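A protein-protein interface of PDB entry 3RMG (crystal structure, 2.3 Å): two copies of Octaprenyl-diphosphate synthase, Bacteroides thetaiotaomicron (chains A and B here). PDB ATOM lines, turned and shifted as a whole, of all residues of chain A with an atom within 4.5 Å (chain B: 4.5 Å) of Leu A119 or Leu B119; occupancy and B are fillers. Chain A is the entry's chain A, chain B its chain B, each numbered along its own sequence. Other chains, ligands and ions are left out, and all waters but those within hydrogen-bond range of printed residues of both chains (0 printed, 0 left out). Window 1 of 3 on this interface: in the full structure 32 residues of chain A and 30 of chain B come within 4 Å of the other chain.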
ATOM      1  N   LEU A  79      -2.451  -7.529   8.116  1.00  0.00           N
ATOM      2  CA  LEU A  79      -2.758  -6.096   8.186  1.00  0.00           C
ATOM      3  C   LEU A  79      -4.128  -5.869   8.830  1.00  0.00           C
ATOM      4  O   LEU A  79      -4.295  -5.001   9.692  1.00  0.00           O
ATOM      5  CB  LEU A  79      -2.712  -5.469   6.786  1.00  0.00           C
ATOM      6  CG  LEU A  79      -3.173  -4.018   6.637  1.00  0.00           C
ATOM      7  CD1 LEU A  79      -2.388  -3.128   7.568  1.00  0.00           C
ATOM      8  CD2 LEU A  79      -2.987  -3.558   5.205  1.00  0.00           C
ATOM      9  N   ALA A  82      -4.031  -6.778  12.523  1.00  0.00           N
ATOM     10  CA  ALA A  82      -3.350  -5.750  13.302  1.00  0.00           C
ATOM     11  C   ALA A  82      -4.243  -4.539  13.595  1.00  0.00           C
ATOM     12  O   ALA A  82      -4.187  -3.974  14.679  1.00  0.00           O
ATOM     13  CB  ALA A  82      -2.054  -5.316  12.620  1.00  0.00           C
ATOM     14  N   GLY A 115       0.071  -5.486  17.907  1.00  0.00           N
ATOM     15  CA  GLY A 115      -0.401  -4.887  16.668  1.00  0.00           C
ATOM     16  C   GLY A 115       0.729  -4.407  15.778  1.00  0.00           C
ATOM     17  O   GLY A 115       0.694  -4.614  14.566  1.00  0.00           O
ATOM     18  N   ASP A 116       1.739  -3.764  16.364  1.00  0.00           N
ATOM     19  CA  ASP A 116       2.858  -3.255  15.566  1.00  0.00           C
ATOM     20  C   ASP A 116       3.665  -4.416  14.969  1.00  0.00           C
ATOM     21  O   ASP A 116       4.174  -4.323  13.847  1.00  0.00           O
ATOM     22  CB  ASP A 116       3.768  -2.332  16.392  1.00  0.00           C
ATOM     23  CG  ASP A 116       3.123  -0.982  16.702  1.00  0.00           C
ATOM     24  OD1 ASP A 116       2.000  -0.727  16.213  1.00  0.00           O
ATOM     25  OD2 ASP A 116       3.747  -0.172  17.438  1.00  0.00           O
ATOM     26  N   TYR A 117       3.782  -5.502  15.730  1.00  0.00           N
ATOM     27  CA  TYR A 117       4.437  -6.713  15.246  1.00  0.00           C
ATOM     28  C   TYR A 117       3.664  -7.303  14.073  1.00  0.00           C
ATOM     29  O   TYR A 117       4.179  -7.371  12.953  1.00  0.00           O
ATOM     30  CB  TYR A 117       4.551  -7.757  16.357  1.00  0.00           C
ATOM     31  CG  TYR A 117       5.394  -8.946  15.963  1.00  0.00           C
ATOM     32  CD1 TYR A 117       6.739  -8.788  15.661  1.00  0.00           C
ATOM     33  CD2 TYR A 117       4.851 -10.222  15.895  1.00  0.00           C
ATOM     34  CE1 TYR A 117       7.523  -9.862  15.299  1.00  0.00           C
ATOM     35  CE2 TYR A 117       5.629 -11.310  15.536  1.00  0.00           C
ATOM     36  CZ  TYR A 117       6.967 -11.120  15.236  1.00  0.00           C
ATOM     37  OH  TYR A 117       7.760 -12.189  14.875  1.00  0.00           O
ATOM     38  N   LEU A 118       2.426  -7.725  14.331  1.00  0.00           N
ATOM     39  CA  LEU A 118       1.562  -8.218  13.256  1.00  0.00           C
ATOM     40  C   LEU A 118       1.705  -7.340  12.019  1.00  0.00           C
ATOM     41  O   LEU A 118       1.825  -7.836  10.899  1.00  0.00           O
ATOM     42  CB  LEU A 118       0.108  -8.268  13.708  1.00  0.00           C
ATOM     43  CG  LEU A 118      -0.172  -9.340  14.762  1.00  0.00           C
ATOM     44  CD1 LEU A 118      -1.449  -9.041  15.535  1.00  0.00           C
ATOM     45  CD2 LEU A 118      -0.247 -10.706  14.112  1.00  0.00           C
ATOM     46  N   LEU A 119       1.732  -6.032  12.240  1.00  0.00           N
ATOM     47  CA  LEU A 119       1.846  -5.043  11.167  1.00  0.00           C
ATOM     48  C   LEU A 119       3.186  -5.102  10.432  1.00  0.00           C
ATOM     49  O   LEU A 119       3.263  -4.896   9.216  1.00  0.00           O
ATOM     50  CB  LEU A 119       1.652  -3.661  11.771  1.00  0.00           C
ATOM     51  CG  LEU A 119       1.142  -2.506  10.930  1.00  0.00           C
ATOM     52  CD1 LEU A 119      -0.263  -2.801  10.434  1.00  0.00           C
ATOM     53  CD2 LEU A 119       1.138  -1.271  11.806  1.00  0.00           C
ATOM     54  N   ALA A 120       4.256  -5.364  11.171  1.00  0.00           N
ATOM     55  CA  ALA A 120       5.561  -5.535  10.542  1.00  0.00           C
ATOM     56  C   ALA A 120       5.598  -6.888   9.844  1.00  0.00           C
ATOM     57  O   ALA A 120       6.024  -7.006   8.695  1.00  0.00           O
ATOM     58  CB  ALA A 120       6.675  -5.435  11.581  1.00  0.00           C
ATOM     59  N   THR A 121       5.153  -7.922  10.542  1.00  0.00           N
ATOM     60  CA  THR A 121       5.108  -9.236   9.920  1.00  0.00           C
ATOM     61  C   THR A 121       4.303  -9.117   8.615  1.00  0.00           C
ATOM     62  O   THR A 121       4.740  -9.597   7.553  1.00  0.00           O
ATOM     63  CB  THR A 121       4.538 -10.293  10.858  1.00  0.00           C
ATOM     64  OG1 THR A 121       5.306 -10.300  12.071  1.00  0.00           O
ATOM     65  CG2 THR A 121       4.611 -11.677  10.210  1.00  0.00           C
ATOM     66  N   SER A 122       3.163  -8.429   8.675  1.00  0.00           N
ATOM     67  CA  SER A 122       2.382  -8.177   7.464  1.00  0.00           C
ATOM     68  C   SER A 122       3.272  -7.667   6.334  1.00  0.00           C
ATOM     69  O   SER A 122       3.167  -8.137   5.195  1.00  0.00           O
ATOM     70  CB  SER A 122       1.251  -7.185   7.738  1.00  0.00           C
ATOM     71  OG  SER A 122       0.294  -7.747   8.618  1.00  0.00           O
ATOM     72  N   LEU A 123       4.161  -6.723   6.647  1.00  0.00           N
ATOM     73  CA  LEU A 123       5.061  -6.146   5.629  1.00  0.00           C
ATOM     74  C   LEU A 123       6.119  -7.111   5.080  1.00  0.00           C
ATOM     75  O   LEU A 123       6.460  -7.081   3.882  1.00  0.00           O
ATOM     76  CB  LEU A 123       5.733  -4.884   6.181  1.00  0.00           C
ATOM     77  N   LEU B  79      10.125   5.117  10.792  1.00  0.00           N
ATOM     78  CA  LEU B  79      10.027   3.931  11.643  1.00  0.00           C
ATOM     79  C   LEU B  79      10.431   4.288  13.079  1.00  0.00           C
ATOM     80  O   LEU B  79       9.754   3.945  14.047  1.00  0.00           O
ATOM     81  CB  LEU B  79      10.929   2.816  11.104  1.00  0.00           C
ATOM     82  CG  LEU B  79      10.928   1.506  11.879  1.00  0.00           C
ATOM     83  CD1 LEU B  79       9.509   1.006  12.027  1.00  0.00           C
ATOM     84  CD2 LEU B  79      11.767   0.469  11.170  1.00  0.00           C
ATOM     85  N   ALA B  82       7.695   6.533  14.770  1.00  0.00           N
ATOM     86  CA  ALA B  82       6.470   5.816  15.159  1.00  0.00           C
ATOM     87  C   ALA B  82       6.621   5.002  16.443  1.00  0.00           C
ATOM     88  O   ALA B  82       5.700   4.947  17.269  1.00  0.00           O
ATOM     89  CB  ALA B  82       5.989   4.923  14.036  1.00  0.00           C
ATOM     90  N   GLY B 115       1.011   6.978  15.417  1.00  0.00           N
ATOM     91  CA  GLY B 115       2.057   5.974  15.298  1.00  0.00           C
ATOM     92  C   GLY B 115       1.828   5.103  14.087  1.00  0.00           C
ATOM     93  O   GLY B 115       2.732   4.918  13.271  1.00  0.00           O
ATOM     94  N   ASP B 116       0.613   4.572  13.962  1.00  0.00           N
ATOM     95  CA  ASP B 116       0.316   3.589  12.917  1.00  0.00           C
ATOM     96  C   ASP B 116       0.479   4.204  11.536  1.00  0.00           C
ATOM     97  O   ASP B 116       0.948   3.559  10.598  1.00  0.00           O
ATOM     98  CB  ASP B 116      -1.090   3.010  13.091  1.00  0.00           C
ATOM     99  CG  ASP B 116      -1.161   1.959  14.192  1.00  0.00           C
ATOM    100  OD1 ASP B 116      -0.145   1.712  14.884  1.00  0.00           O
ATOM    101  OD2 ASP B 116      -2.250   1.377  14.369  1.00  0.00           O
ATOM    102  N   TYR B 117       0.094   5.467  11.427  1.00  0.00           N
ATOM    103  CA  TYR B 117       0.283   6.221  10.203  1.00  0.00           C
ATOM    104  C   TYR B 117       1.762   6.304   9.826  1.00  0.00           C
ATOM    105  O   TYR B 117       2.184   5.755   8.804  1.00  0.00           O
ATOM    106  CB  TYR B 117      -0.291   7.623  10.365  1.00  0.00           C
ATOM    107  CG  TYR B 117      -0.279   8.401   9.078  1.00  0.00           C
ATOM    108  CD1 TYR B 117      -0.852   7.872   7.927  1.00  0.00           C
ATOM    109  CD2 TYR B 117       0.306   9.658   9.009  1.00  0.00           C
ATOM    110  CE1 TYR B 117      -0.846   8.569   6.750  1.00  0.00           C
ATOM    111  CE2 TYR B 117       0.315  10.366   7.831  1.00  0.00           C
ATOM    112  CZ  TYR B 117      -0.259   9.815   6.704  1.00  0.00           C
ATOM    113  OH  TYR B 117      -0.249  10.518   5.522  1.00  0.00           O
ATOM    114  N   LEU B 118       2.547   6.984  10.658  1.00  0.00           N
ATOM    115  CA  LEU B 118       3.985   7.114  10.418  1.00  0.00           C
ATOM    116  C   LEU B 118       4.586   5.773  10.012  1.00  0.00           C
ATOM    117  O   LEU B 118       5.404   5.693   9.097  1.00  0.00           O
ATOM    118  CB  LEU B 118       4.674   7.637  11.670  1.00  0.00           C
ATOM    119  CG  LEU B 118       4.120   8.985  12.124  1.00  0.00           C
ATOM    120  CD1 LEU B 118       4.788   9.433  13.402  1.00  0.00           C
ATOM    121  CD2 LEU B 118       4.304  10.018  11.026  1.00  0.00           C
ATOM    122  N   LEU B 119       4.144   4.721  10.694  1.00  0.00           N
ATOM    123  CA  LEU B 119       4.585   3.360  10.435  1.00  0.00           C
ATOM    124  C   LEU B 119       4.276   2.919   9.010  1.00  0.00           C
ATOM    125  O   LEU B 119       5.121   2.338   8.316  1.00  0.00           O
ATOM    126  CB  LEU B 119       3.886   2.428  11.417  1.00  0.00           C
ATOM    127  CG  LEU B 119       4.491   1.066  11.708  1.00  0.00           C
ATOM    128  CD1 LEU B 119       5.900   1.259  12.232  1.00  0.00           C
ATOM    129  CD2 LEU B 119       3.617   0.371  12.742  1.00  0.00           C
ATOM    130  N   ALA B 120       3.048   3.174   8.574  1.00  0.00           N
ATOM    131  CA  ALA B 120       2.646   2.780   7.231  1.00  0.00           C
ATOM    132  C   ALA B 120       3.396   3.636   6.202  1.00  0.00           C
ATOM    133  O   ALA B 120       3.868   3.126   5.186  1.00  0.00           O
ATOM    134  CB  ALA B 120       1.142   2.904   7.067  1.00  0.00           C
ATOM    135  N   THR B 121       3.526   4.930   6.490  1.00  0.00           N
ATOM    136  CA  THR B 121       4.338   5.827   5.659  1.00  0.00           C
ATOM    137  C   THR B 121       5.810   5.376   5.545  1.00  0.00           C
ATOM    138  O   THR B 121       6.440   5.561   4.500  1.00  0.00           O
ATOM    139  CB  THR B 121       4.265   7.276   6.168  1.00  0.00           C
ATOM    140  OG1 THR B 121       2.903   7.603   6.464  1.00  0.00           O
ATOM    141  CG2 THR B 121       4.802   8.243   5.116  1.00  0.00           C
ATOM    142  N   SER B 122       6.349   4.777   6.606  1.00  0.00           N
ATOM    143  CA  SER B 122       7.701   4.223   6.565  1.00  0.00           C
ATOM    144  C   SER B 122       7.853   3.168   5.475  1.00  0.00           C
ATOM    145  O   SER B 122       8.772   3.242   4.644  1.00  0.00           O
ATOM    146  CB  SER B 122       8.076   3.621   7.919  1.00  0.00           C
ATOM    147  OG  SER B 122       8.150   4.627   8.910  1.00  0.00           O
ATOM    148  N   LEU B 123       6.956   2.181   5.484  1.00  0.00           N
ATOM    149  CA  LEU B 123       6.980   1.104   4.495  1.00  0.00           C
ATOM    150  C   LEU B 123       6.799   1.646   3.077  1.00  0.00           C
ATOM    151  O   LEU B 123       7.342   1.093   2.096  1.00  0.00           O
ATOM    152  CB  LEU B 123       5.902   0.059   4.816  1.00  0.00           C
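OD1 of Asp B116 touches OD1 of Asp A116, at 3.5 Å.
CD2 of Leu B119 touches OD1 of Asp A116, at 3.98 Å.
Leu A119 touches Leu B119.
Hydrophobic or aromatic side chains of chain A that line the printed part of chain B: Leu A119.
Hydrophobic or aromatic side chains of chain B that line the printed part of chain A: Leu B119.
Along chain B the printed residues that touch a printed residue of chain A span positions 116 to 119.
Among the printed residues, no Asp or Glu carboxylate lies within 4 Å of a Lys or Arg side-chain nitrogen of the other chain.
Of the printed residues of chain B, Asp A116 touches Asp B116 (3.5 Å) and Leu B119 (3.98 Å).
Leu A119 touches just one residue of chain B: Leu B119 (3.1 Å).
Leu B79 touches none of the printed residues of chain A.
Of the printed residues of chain A, Asp B116 touches Asp A116 (3.5 Å).
Of the printed residues of chain A, Leu B119 touches Asp A116 (3.98 Å) and Leu A119 (3.1 Å).
Ser B122 touches none of the printed residues of chain A.
The nearest printed residue of chain A that does not touch Asp B116 is Leu A119 (4.5 Å).
Asp B116 touches its own counterpart, Asp A116.
Asp A116 touches Leu B119, but with the chains exchanged Leu A119 does not touch Asp B116 (4.5 Å).
Leu B119 touches its own counterpart, Leu A119.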
